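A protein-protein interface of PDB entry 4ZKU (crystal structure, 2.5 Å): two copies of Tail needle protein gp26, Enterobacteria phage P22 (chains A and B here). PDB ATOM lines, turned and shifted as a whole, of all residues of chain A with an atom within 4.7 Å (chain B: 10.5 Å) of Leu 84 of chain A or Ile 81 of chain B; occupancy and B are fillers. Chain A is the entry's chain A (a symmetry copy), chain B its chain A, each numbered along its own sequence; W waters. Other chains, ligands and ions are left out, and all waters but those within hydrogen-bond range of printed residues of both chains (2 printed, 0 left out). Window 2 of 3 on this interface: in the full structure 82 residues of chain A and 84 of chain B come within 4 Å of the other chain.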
ATOM      1  N   HIS A  77     -21.849 -35.147  25.906  1.00  0.00           N
ATOM      2  CA  HIS A  77     -20.782 -34.314  25.365  1.00  0.00           C
ATOM      3  C   HIS A  77     -20.969 -34.096  23.867  1.00  0.00           C
ATOM      4  O   HIS A  77     -20.776 -32.990  23.367  1.00  0.00           O
ATOM      5  CB  HIS A  77     -19.415 -34.941  25.642  1.00  0.00           C
ATOM      6  CG  HIS A  77     -18.955 -34.792  27.063  1.00  0.00           C
ATOM      7  ND1 HIS A  77     -17.716 -35.203  27.488  1.00  0.00           N
ATOM      8  CD2 HIS A  77     -19.579 -34.269  28.146  1.00  0.00           C
ATOM      9  CE1 HIS A  77     -17.589 -34.943  28.781  1.00  0.00           C
ATOM     10  NE2 HIS A  77     -18.701 -34.379  29.201  1.00  0.00           N
ATOM     11  N   ARG A  80     -23.627 -31.565  23.200  1.00  0.00           N
ATOM     12  CA  ARG A  80     -23.220 -30.231  23.628  1.00  0.00           C
ATOM     13  C   ARG A  80     -22.199 -29.605  22.681  1.00  0.00           C
ATOM     14  O   ARG A  80     -22.197 -28.391  22.480  1.00  0.00           O
ATOM     15  CB  ARG A  80     -22.663 -30.290  25.052  1.00  0.00           C
ATOM     16  CG  ARG A  80     -23.744 -30.369  26.116  1.00  0.00           C
ATOM     17  CD  ARG A  80     -23.205 -30.912  27.429  1.00  0.00           C
ATOM     18  NE  ARG A  80     -22.377 -29.940  28.136  1.00  0.00           N
ATOM     19  CZ  ARG A  80     -21.581 -30.245  29.155  1.00  0.00           C
ATOM     20  NH1 ARG A  80     -21.506 -31.498  29.583  1.00  0.00           N
ATOM     21  NH2 ARG A  80     -20.861 -29.301  29.749  1.00  0.00           N
ATOM     22  N   ILE A  81     -21.328 -30.429  22.108  1.00  0.00           N
ATOM     23  CA  ILE A  81     -20.358 -29.948  21.128  1.00  0.00           C
ATOM     24  C   ILE A  81     -21.085 -29.518  19.859  1.00  0.00           C
ATOM     25  O   ILE A  81     -20.740 -28.504  19.252  1.00  0.00           O
ATOM     26  CB  ILE A  81     -19.286 -31.010  20.819  1.00  0.00           C
ATOM     27  CG1 ILE A  81     -18.453 -31.309  22.068  1.00  0.00           C
ATOM     28  CG2 ILE A  81     -18.381 -30.547  19.686  1.00  0.00           C
ATOM     29  CD1 ILE A  81     -17.575 -32.531  21.937  1.00  0.00           C
ATOM     30  N   LYS A  82     -22.095 -30.291  19.466  1.00  0.00           N
ATOM     31  CA  LYS A  82     -22.904 -29.953  18.297  1.00  0.00           C
ATOM     32  C   LYS A  82     -23.551 -28.582  18.436  1.00  0.00           C
ATOM     33  O   LYS A  82     -23.514 -27.776  17.508  1.00  0.00           O
ATOM     34  CB  LYS A  82     -23.992 -31.003  18.059  1.00  0.00           C
ATOM     35  CG  LYS A  82     -23.531 -32.246  17.326  1.00  0.00           C
ATOM     36  CD  LYS A  82     -24.710 -32.920  16.642  1.00  0.00           C
ATOM     37  CE  LYS A  82     -24.302 -34.202  15.942  1.00  0.00           C
ATOM     38  NZ  LYS A  82     -24.110 -35.326  16.897  1.00  0.00           N
ATOM     39  N   GLN A  83     -24.136 -28.317  19.599  1.00  0.00           N
ATOM     40  CA  GLN A  83     -24.835 -27.058  19.817  1.00  0.00           C
ATOM     41  C   GLN A  83     -23.852 -25.893  19.895  1.00  0.00           C
ATOM     42  O   GLN A  83     -24.136 -24.804  19.398  1.00  0.00           O
ATOM     43  CB  GLN A  83     -25.684 -27.125  21.086  1.00  0.00           C
ATOM     44  CG  GLN A  83     -26.594 -25.925  21.266  1.00  0.00           C
ATOM     45  CD  GLN A  83     -27.522 -25.724  20.083  1.00  0.00           C
ATOM     46  OE1 GLN A  83     -28.323 -26.598  19.752  1.00  0.00           O
ATOM     47  NE2 GLN A  83     -27.416 -24.570  19.436  1.00  0.00           N
ATOM     48  N   LEU A  84     -22.704 -26.126  20.526  1.00  0.00           N
ATOM     49  CA  LEU A  84     -21.639 -25.130  20.570  1.00  0.00           C
ATOM     50  C   LEU A  84     -21.175 -24.799  19.158  1.00  0.00           C
ATOM     51  O   LEU A  84     -20.972 -23.635  18.815  1.00  0.00           O
ATOM     52  CB  LEU A  84     -20.457 -25.627  21.405  1.00  0.00           C
ATOM     53  CG  LEU A  84     -20.542 -25.498  22.925  1.00  0.00           C
ATOM     54  CD1 LEU A  84     -19.362 -26.196  23.585  1.00  0.00           C
ATOM     55  CD2 LEU A  84     -20.600 -24.037  23.338  1.00  0.00           C
ATOM     56  N   ARG A  85     -21.015 -25.839  18.346  1.00  0.00           N
ATOM     57  CA  ARG A  85     -20.579 -25.690  16.963  1.00  0.00           C
ATOM     58  C   ARG A  85     -21.590 -24.878  16.159  1.00  0.00           C
ATOM     59  O   ARG A  85     -21.215 -24.063  15.319  1.00  0.00           O
ATOM     60  CB  ARG A  85     -20.364 -27.063  16.324  1.00  0.00           C
ATOM     61  CG  ARG A  85     -19.724 -27.040  14.944  1.00  0.00           C
ATOM     62  CD  ARG A  85     -18.264 -26.609  14.997  1.00  0.00           C
ATOM     63  NE  ARG A  85     -18.106 -25.167  14.840  1.00  0.00           N
ATOM     64  CZ  ARG A  85     -16.957 -24.519  15.009  1.00  0.00           C
ATOM     65  NH1 ARG A  85     -15.863 -25.184  15.348  1.00  0.00           N
ATOM     66  NH2 ARG A  85     -16.906 -23.205  14.841  1.00  0.00           N
ATOM     67  N   ILE A  86     -22.872 -25.105  16.427  1.00  0.00           N
ATOM     68  CA  ILE A  86     -23.939 -24.363  15.765  1.00  0.00           C
ATOM     69  C   ILE A  86     -23.864 -22.886  16.136  1.00  0.00           C
ATOM     70  O   ILE A  86     -23.977 -22.012  15.275  1.00  0.00           O
ATOM     71  CB  ILE A  86     -25.324 -24.943  16.121  1.00  0.00           C
ATOM     72  CG1 ILE A  86     -25.493 -26.340  15.521  1.00  0.00           C
ATOM     73  CG2 ILE A  86     -26.435 -24.022  15.643  1.00  0.00           C
ATOM     74  CD1 ILE A  86     -26.829 -26.979  15.834  1.00  0.00           C
ATOM     75  N   ASP A  87     -23.660 -22.617  17.421  1.00  0.00           N
ATOM     76  CA  ASP A  87     -23.617 -21.250  17.929  1.00  0.00           C
ATOM     77  C   ASP A  87     -22.397 -20.482  17.428  1.00  0.00           C
ATOM     78  O   ASP A  87     -22.506 -19.318  17.042  1.00  0.00           O
ATOM     79  CB  ASP A  87     -23.640 -21.255  19.459  1.00  0.00           C
ATOM     80  CG  ASP A  87     -24.880 -21.923  20.021  1.00  0.00           C
ATOM     81  OD1 ASP A  87     -25.869 -22.068  19.272  1.00  0.00           O
ATOM     82  OD2 ASP A  87     -24.866 -22.306  21.211  1.00  0.00           O
ATOM     83  N   VAL A  88     -21.238 -21.133  17.441  1.00  0.00           N
ATOM     84  CA  VAL A  88     -19.999 -20.485  17.032  1.00  0.00           C
ATOM     85  C   VAL A  88     -19.989 -20.237  15.524  1.00  0.00           C
ATOM     86  O   VAL A  88     -19.507 -19.201  15.061  1.00  0.00           O
ATOM     87  CB  VAL A  88     -18.773 -21.315  17.465  1.00  0.00           C
ATOM     88  CG1 VAL A  88     -17.494 -20.721  16.899  1.00  0.00           C
ATOM     89  CG2 VAL A  88     -18.696 -21.393  18.980  1.00  0.00           C
ATOM     90  N   GLU B  73     -10.231 -38.125  31.207  1.00  0.00           N
ATOM     91  CA  GLU B  73     -10.384 -37.385  29.961  1.00  0.00           C
ATOM     92  C   GLU B  73     -11.816 -36.873  29.809  1.00  0.00           C
ATOM     93  O   GLU B  73     -12.039 -35.773  29.304  1.00  0.00           O
ATOM     94  CB  GLU B  73      -9.993 -38.268  28.772  1.00  0.00           C
ATOM     95  CG  GLU B  73     -10.163 -37.615  27.412  1.00  0.00           C
ATOM     96  CD  GLU B  73      -9.556 -38.444  26.295  1.00  0.00           C
ATOM     97  OE1 GLU B  73      -9.444 -37.929  25.161  1.00  0.00           O
ATOM     98  OE2 GLU B  73      -9.185 -39.610  26.554  1.00  0.00           O
ATOM     99  N   LEU B  74     -12.779 -37.676  30.250  1.00  0.00           N
ATOM    100  CA  LEU B  74     -14.180 -37.262  30.261  1.00  0.00           C
ATOM    101  C   LEU B  74     -14.395 -36.060  31.173  1.00  0.00           C
ATOM    102  O   LEU B  74     -15.163 -35.154  30.851  1.00  0.00           O
ATOM    103  CB  LEU B  74     -15.083 -38.416  30.702  1.00  0.00           C
ATOM    104  CG  LEU B  74     -15.423 -39.472  29.652  1.00  0.00           C
ATOM    105  CD1 LEU B  74     -16.210 -40.606  30.280  1.00  0.00           C
ATOM    106  CD2 LEU B  74     -16.202 -38.846  28.509  1.00  0.00           C
ATOM    107  N   ALA B  75     -13.714 -36.061  32.316  1.00  0.00           N
ATOM    108  CA  ALA B  75     -13.804 -34.960  33.266  1.00  0.00           C
ATOM    109  C   ALA B  75     -13.164 -33.700  32.690  1.00  0.00           C
ATOM    110  O   ALA B  75     -13.632 -32.589  32.933  1.00  0.00           O
ATOM    111  CB  ALA B  75     -13.147 -35.338  34.586  1.00  0.00           C
ATOM    112  N   ASP B  76     -12.092 -33.886  31.927  1.00  0.00           N
ATOM    113  CA  ASP B  76     -11.395 -32.770  31.299  1.00  0.00           C
ATOM    114  C   ASP B  76     -12.261 -32.152  30.208  1.00  0.00           C
ATOM    115  O   ASP B  76     -12.395 -30.931  30.125  1.00  0.00           O
ATOM    116  CB  ASP B  76     -10.057 -33.226  30.716  1.00  0.00           C
ATOM    117  CG  ASP B  76      -9.334 -32.115  29.982  1.00  0.00           C
ATOM    118  OD1 ASP B  76      -9.108 -31.049  30.590  1.00  0.00           O
ATOM    119  OD2 ASP B  76      -8.996 -32.307  28.795  1.00  0.00           O
ATOM    120  N   HIS B  77     -12.840 -33.008  29.372  1.00  0.00           N
ATOM    121  CA  HIS B  77     -13.754 -32.568  28.325  1.00  0.00           C
ATOM    122  C   HIS B  77     -14.953 -31.839  28.923  1.00  0.00           C
ATOM    123  O   HIS B  77     -15.390 -30.817  28.398  1.00  0.00           O
ATOM    124  CB  HIS B  77     -14.220 -33.755  27.483  1.00  0.00           C
ATOM    125  CG  HIS B  77     -13.189 -34.258  26.517  1.00  0.00           C
ATOM    126  ND1 HIS B  77     -13.447 -35.254  25.607  1.00  0.00           N
ATOM    127  CD2 HIS B  77     -11.899 -33.888  26.325  1.00  0.00           C
ATOM    128  CE1 HIS B  77     -12.357 -35.484  24.890  1.00  0.00           C
ATOM    129  NE2 HIS B  77     -11.409 -34.672  25.305  1.00  0.00           N
ATOM    130  N   GLU B  78     -15.478 -32.372  30.023  1.00  0.00           N
ATOM    131  CA  GLU B  78     -16.638 -31.787  30.685  1.00  0.00           C
ATOM    132  C   GLU B  78     -16.342 -30.364  31.153  1.00  0.00           C
ATOM    133  O   GLU B  78     -17.172 -29.467  31.012  1.00  0.00           O
ATOM    134  CB  GLU B  78     -17.070 -32.650  31.872  1.00  0.00           C
ATOM    135  CG  GLU B  78     -18.169 -32.024  32.713  1.00  0.00           C
ATOM    136  CD  GLU B  78     -19.466 -31.863  31.944  1.00  0.00           C
ATOM    137  OE1 GLU B  78     -20.159 -30.844  32.151  1.00  0.00           O
ATOM    138  OE2 GLU B  78     -19.786 -32.751  31.124  1.00  0.00           O
ATOM    139  N   ALA B  79     -15.152 -30.170  31.710  1.00  0.00           N
ATOM    140  CA  ALA B  79     -14.743 -28.863  32.208  1.00  0.00           C
ATOM    141  C   ALA B  79     -14.563 -27.874  31.061  1.00  0.00           C
ATOM    142  O   ALA B  79     -14.883 -26.693  31.188  1.00  0.00           O
ATOM    143  CB  ALA B  79     -13.457 -28.982  33.013  1.00  0.00           C
ATOM    144  N   ARG B  80     -14.046 -28.368  29.940  1.00  0.00           N
ATOM    145  CA  ARG B  80     -13.755 -27.526  28.786  1.00  0.00           C
ATOM    146  C   ARG B  80     -15.020 -27.118  28.032  1.00  0.00           C
ATOM    147  O   ARG B  80     -15.094 -26.017  27.488  1.00  0.00           O
ATOM    148  CB  ARG B  80     -12.785 -28.247  27.849  1.00  0.00           C
ATOM    149  CG  ARG B  80     -11.343 -28.198  28.324  1.00  0.00           C
ATOM    150  CD  ARG B  80     -10.501 -29.293  27.690  1.00  0.00           C
ATOM    151  NE  ARG B  80     -10.199 -29.022  26.288  1.00  0.00           N
ATOM    152  CZ  ARG B  80      -9.718 -29.928  25.445  1.00  0.00           C
ATOM    153  NH1 ARG B  80      -9.486 -31.164  25.864  1.00  0.00           N
ATOM    154  NH2 ARG B  80      -9.465 -29.601  24.183  1.00  0.00           N
ATOM    155  N   ILE B  81     -16.008 -28.006  27.994  1.00  0.00           N
ATOM    156  CA  ILE B  81     -17.288 -27.692  27.367  1.00  0.00           C
ATOM    157  C   ILE B  81     -18.010 -26.629  28.188  1.00  0.00           C
ATOM    158  O   ILE B  81     -18.621 -25.715  27.633  1.00  0.00           O
ATOM    159  CB  ILE B  81     -18.163 -28.948  27.194  1.00  0.00           C
ATOM    160  CG1 ILE B  81     -17.497 -29.935  26.232  1.00  0.00           C
ATOM    161  CG2 ILE B  81     -19.546 -28.574  26.685  1.00  0.00           C
ATOM    162  CD1 ILE B  81     -18.136 -31.304  26.225  1.00  0.00           C
ATOM    163  N   LYS B  82     -17.935 -26.752  29.511  1.00  0.00           N
ATOM    164  CA  LYS B  82     -18.538 -25.767  30.404  1.00  0.00           C
ATOM    165  C   LYS B  82     -17.991 -24.368  30.154  1.00  0.00           C
ATOM    166  O   LYS B  82     -18.751 -23.406  30.064  1.00  0.00           O
ATOM    167  CB  LYS B  82     -18.312 -26.142  31.871  1.00  0.00           C
ATOM    168  CG  LYS B  82     -19.279 -27.170  32.424  1.00  0.00           C
ATOM    169  CD  LYS B  82     -19.367 -27.048  33.937  1.00  0.00           C
ATOM    170  CE  LYS B  82     -20.282 -28.097  34.537  1.00  0.00           C
ATOM    171  NZ  LYS B  82     -19.635 -29.435  34.603  1.00  0.00           N
ATOM    172  N   GLN B  83     -16.672 -24.260  30.035  1.00  0.00           N
ATOM    173  CA  GLN B  83     -16.041 -22.961  29.852  1.00  0.00           C
ATOM    174  C   GLN B  83     -16.345 -22.393  28.469  1.00  0.00           C
ATOM    175  O   GLN B  83     -16.552 -21.190  28.320  1.00  0.00           O
ATOM    176  CB  GLN B  83     -14.530 -23.060  30.065  1.00  0.00           C
ATOM    177  CG  GLN B  83     -13.835 -21.713  30.091  1.00  0.00           C
ATOM    178  CD  GLN B  83     -14.405 -20.790  31.152  1.00  0.00           C
ATOM    179  OE1 GLN B  83     -14.384 -21.106  32.341  1.00  0.00           O
ATOM    180  NE2 GLN B  83     -14.924 -19.646  30.724  1.00  0.00           N
ATOM    181  N   LEU B  84     -16.365 -23.263  27.462  1.00  0.00           N
ATOM    182  CA  LEU B  84     -16.755 -22.863  26.114  1.00  0.00           C
ATOM    183  C   LEU B  84     -18.182 -22.334  26.117  1.00  0.00           C
ATOM    184  O   LEU B  84     -18.480 -21.315  25.495  1.00  0.00           O
ATOM    185  CB  LEU B  84     -16.636 -24.036  25.138  1.00  0.00           C
ATOM    186  CG  LEU B  84     -15.256 -24.362  24.566  1.00  0.00           C
ATOM    187  CD1 LEU B  84     -15.305 -25.651  23.760  1.00  0.00           C
ATOM    188  CD2 LEU B  84     -14.744 -23.215  23.711  1.00  0.00           C
ATOM    189  N   ARG B  85     -19.056 -23.039  26.828  1.00  0.00           N
ATOM    190  CA  ARG B  85     -20.460 -22.663  26.935  1.00  0.00           C
ATOM    191  C   ARG B  85     -20.607 -21.301  27.607  1.00  0.00           C
ATOM    192  O   ARG B  85     -21.453 -20.498  27.217  1.00  0.00           O
ATOM    193  CB  ARG B  85     -21.237 -23.730  27.709  1.00  0.00           C
ATOM    194  CG  ARG B  85     -22.747 -23.547  27.721  1.00  0.00           C
ATOM    195  CD  ARG B  85     -23.366 -23.797  26.353  1.00  0.00           C
ATOM    196  NE  ARG B  85     -23.457 -22.579  25.555  1.00  0.00           N
ATOM    197  CZ  ARG B  85     -23.805 -22.552  24.272  1.00  0.00           C
ATOM    198  NH1 ARG B  85     -24.092 -23.678  23.635  1.00  0.00           N
ATOM    199  NH2 ARG B  85     -23.867 -21.396  23.625  1.00  0.00           N
ATOM    200  N   ILE B  86     -19.778 -21.048  28.614  1.00  0.00           N
ATOM    201  CA  ILE B  86     -19.780 -19.768  29.311  1.00  0.00           C
ATOM    202  C   ILE B  86     -19.369 -18.648  28.360  1.00  0.00           C
ATOM    203  O   ILE B  86     -19.992 -17.587  28.326  1.00  0.00           O
ATOM    204  CB  ILE B  86     -18.854 -19.802  30.544  1.00  0.00           C
ATOM    205  CG1 ILE B  86     -19.415 -20.742  31.612  1.00  0.00           C
ATOM    206  CG2 ILE B  86     -18.661 -18.406  31.113  1.00  0.00           C
ATOM    207  CD1 ILE B  86     -18.554 -20.835  32.853  1.00  0.00           C
ATOM    208  N   ASP B  87     -18.322 -18.901  27.581  1.00  0.00           N
ATOM    209  CA  ASP B  87     -17.784 -17.905  26.662  1.00  0.00           C
ATOM    210  C   ASP B  87     -18.741 -17.596  25.514  1.00  0.00           C
ATOM    211  O   ASP B  87     -18.929 -16.435  25.150  1.00  0.00           O
ATOM    212  CB  ASP B  87     -16.437 -18.374  26.106  1.00  0.00           C
ATOM    213  CG  ASP B  87     -15.408 -18.608  27.193  1.00  0.00           C
ATOM    214  OD1 ASP B  87     -15.599 -18.091  28.315  1.00  0.00           O
ATOM    215  OD2 ASP B  87     -14.408 -19.311  26.930  1.00  0.00           O
ATOM    216  N   VAL B  88     -19.342 -18.637  24.944  1.00  0.00           N
ATOM    217  CA  VAL B  88     -20.239 -18.467  23.808  1.00  0.00           C
ATOM    218  C   VAL B  88     -21.540 -17.791  24.242  1.00  0.00           C
ATOM    219  O   VAL B  88     -22.088 -16.961  23.515  1.00  0.00           O
ATOM    220  CB  VAL B  88     -20.520 -19.819  23.120  1.00  0.00           C
ATOM    221  CG1 VAL B  88     -21.578 -19.663  22.040  1.00  0.00           C
ATOM    222  CG2 VAL B  88     -19.241 -20.387  22.529  1.00  0.00           C
ATOM    223  N   ASP B  89     -22.022 -18.135  25.433  1.00  0.00           N
ATOM    224  CA  ASP B  89     -23.220 -17.500  25.980  1.00  0.00           C
ATOM    225  C   ASP B  89     -22.996 -16.009  26.204  1.00  0.00           C
ATOM    226  O   ASP B  89     -23.911 -15.201  26.043  1.00  0.00           O
ATOM    227  CB  ASP B  89     -23.639 -18.167  27.293  1.00  0.00           C
ATOM    228  CG  ASP B  89     -24.351 -19.488  27.075  1.00  0.00           C
ATOM    229  OD1 ASP B  89     -24.839 -19.726  25.951  1.00  0.00           O
ATOM    230  OD2 ASP B  89     -24.425 -20.287  28.031  1.00  0.00           O
ATOM    231  N   ASP B  90     -21.771 -15.650  26.571  1.00  0.00           N
ATOM    232  CA  ASP B  90     -21.427 -14.260  26.843  1.00  0.00           C
ATOM    233  C   ASP B  90     -21.163 -13.514  25.540  1.00  0.00           C
ATOM    234  O   ASP B  90     -21.438 -12.318  25.429  1.00  0.00           O
ATOM    235  CB  ASP B  90     -20.211 -14.180  27.768  1.00  0.00           C
ATOM    236  CG  ASP B  90     -19.592 -12.796  27.804  1.00  0.00           C
ATOM    237  OD1 ASP B  90     -20.185 -11.895  28.432  1.00  0.00           O
ATOM    238  OD2 ASP B  90     -18.512 -12.612  27.205  1.00  0.00           O
ATOM    239  N   HIS B  91     -20.629 -14.229  24.554  1.00  0.00           N
ATOM    240  CA  HIS B  91     -20.442 -13.672  23.221  1.00  0.00           C
ATOM    241  C   HIS B  91     -21.786 -13.368  22.576  1.00  0.00           C
ATOM    242  O   HIS B  91     -21.938 -12.361  21.886  1.00  0.00           O
ATOM    243  CB  HIS B  91     -19.644 -14.629  22.335  1.00  0.00           C
ATOM    244  CG  HIS B  91     -18.168 -14.604  22.590  1.00  0.00           C
ATOM    245  ND1 HIS B  91     -17.277 -15.361  21.861  1.00  0.00           N
ATOM    246  CD2 HIS B  91     -17.431 -13.906  23.484  1.00  0.00           C
ATOM    247  CE1 HIS B  91     -16.052 -15.133  22.301  1.00  0.00           C
ATOM    248  NE2 HIS B  91     -16.117 -14.255  23.283  1.00  0.00           N
ATOM    249  N   GLU B  92     -22.752 -14.253  22.805  1.00  0.00           N
ATOM    250  CA  GLU B  92     -24.102 -14.097  22.276  1.00  0.00           C
ATOM    251  C   GLU B  92     -24.675 -12.735  22.657  1.00  0.00           C
ATOM    252  O   GLU B  92     -25.222 -12.022  21.817  1.00  0.00           O
ATOM    253  CB  GLU B  92     -25.009 -15.215  22.789  1.00  0.00           C
ATOM    254  CG  GLU B  92     -26.412 -15.182  22.214  1.00  0.00           C
ATOM    255  CD  GLU B  92     -26.414 -15.303  20.700  1.00  0.00           C
ATOM    256  OE1 GLU B  92     -27.245 -14.642  20.044  1.00  0.00           O
ATOM    257  OE2 GLU B  92     -25.584 -16.070  20.165  1.00  0.00           O
HETATM  258  O   HOH W   1     -16.011 -36.395  25.604  1.00  0.00           O
HETATM  259  O   HOH W   2     -23.705 -26.112  23.713  1.00  0.00           O
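OE2 of Glu 78 of chain B lies within hydrogen-bond range of NE2 of His 77 of chain A.
The side-chain carboxylate (OE2) of Glu 78 of chain B lies within salt-bridge range of the guanidinium group (NH1) of Arg 80 of chain A, 2.6 Å away.
The guanidinium group of Arg 85 of chain B is in salt-bridge range of the side-chain carboxylate of Asp 87 of chain A, at 2.8 Å.
The side-chain amino group (NZ) of Lys 82 of chain B is in salt-bridge range of the side-chain carboxylate (OE1) of Glu 78 of chain B, 2.9 Å away.
The guanidinium group of Arg 85 of chain B lies within salt-bridge range of the side-chain carboxylate of Asp 89 of chain B, 3.0 Å away.
The side-chain amide nitrogen of Gln 83 of chain A lies within hydrogen-bond range of the side-chain carboxylate of Asp 87 of chain A, 2.9 Å away.
Among the printed residues, pairs that only touch across the chains: His 77 of chain A with Leu 74 of chain B (3.2 Å), Arg 80 of chain A with Ile 81 of chain B (3.4 Å), Leu 84 of chain A with Arg 85 of chain B (3.5 Å), Asp 87 of chain A with Val 88 of chain B (3.7 Å), His 77 of chain A with Ile 81 of chain B (3.7 Å), Val 88 of chain A with Val 88 of chain B (3.7 Å), Arg 80 of chain A with Lys 82 of chain B (3.8 Å), His 77 of chain A with His 77 of chain B (3.8 Å), Leu 84 of chain A with Leu 84 of chain B (3.8 Å), Leu 84 of chain A with Ile 81 of chain B (3.9 Å) and Leu 84 of chain A with Val 88 of chain B (3.98 Å).
Printed residues of chain B within 4 Å of His 77 of chain A: Leu 74, His 77, Glu 78 and Ile 81.
Of the printed residues of chain B, Arg 80 of chain A touches Glu 78 (2.6 Å), Ile 81 (3.4 Å) and Lys 82 (3.8 Å).
No residue of chain B comes within 4 Å of Ile 81 of chain A.
Gln 83 of chain A touches none of the printed residues of chain B.
Leu 84 of chain A touches just these residues of chain B: Ile 81 (3.9 Å), Leu 84 (3.8 Å), Arg 85 (3.5 Å) and Val 88 (3.98 Å).
No residue of chain B comes within 4 Å of Ile 86 of chain A.
Printed residues of chain B within 4 Å of Asp 87 of chain A: Arg 85 and Val 88.
Val 88 of chain A touches one residue of chain B.
Of the printed residues of chain A, His 77 of chain B touches His 77 (3.8 Å).
Of the printed residues of chain A, Glu 78 of chain B touches His 77 (2.7 Å) and Arg 80 (2.6 Å).
Ala 79 of chain B touches none of the printed residues of chain A.
Of the printed residues of chain A, Ile 81 of chain B touches His 77 (3.7 Å), Arg 80 (3.4 Å) and Leu 84 (3.9 Å).
Of the printed residues of chain A, Arg 85 of chain B touches Leu 84 (3.5 Å) and Asp 87 (2.8 Å).
His 91 of chain B touches none of the printed residues of chain A.
The nearest residue of chain A that does not touch Ile 81 of chain B is Ile 81 of chain A (4.2 Å).
Of the 20 printed residues of chain B, 8 touch a printed residue of chain A.
Printed residues of chain B that touch a printed residue of chain A: Leu 74, His 77, Glu 78, Ile 81, Lys 82, Leu 84, Arg 85 and Val 88.
Hydrophobic or aromatic side chains of chain B within 4 Å of the printed part of chain A: His 77, Ile 81, Leu 84 and Val 88.
Among the printed residues, Asp or Glu carboxylates within 4 Å of a Lys or Arg side-chain nitrogen of the other chain: Arg 80 of chain A with Glu 78 of chain B (2.6 Å) and Asp 87 of chain A with Arg 85 of chain B (2.8 Å).
His 77 of chain A touches Ile 81 of chain B, but with the chains exchanged Ile 81 of chain A does not touch His 77 of chain B (6.2 Å).
Leu 84 of chain B touches its own counterpart, Leu 84 of chain A.
Leu 84 of chain A touches Arg 85 of chain B, but with the chains exchanged Arg 85 of chain A does not touch Leu 84 of chain B (7.9 Å).
Leu 84 of chain A touches Val 88 of chain B, but with the chains exchanged Val 88 of chain A does not touch Leu 84 of chain B (6.4 Å).
Of the 14 pairs that touch across the chains among the printed residues, 3 have their exchanged pair printed and touching as well.
Water W2 lies within hydrogen-bond range of the guanidinium group of Arg 85 of chain B (2.5 Å), the backbone carbonyl oxygen of Arg 80 of chain A (3.0 Å) and the backbone NH of Leu 84 of chain A (3.3 Å).
Water W1 bridges ND1 of His 77 of chain B (2.8 Å) and ND1 of His 77 of chain A (2.8 Å).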
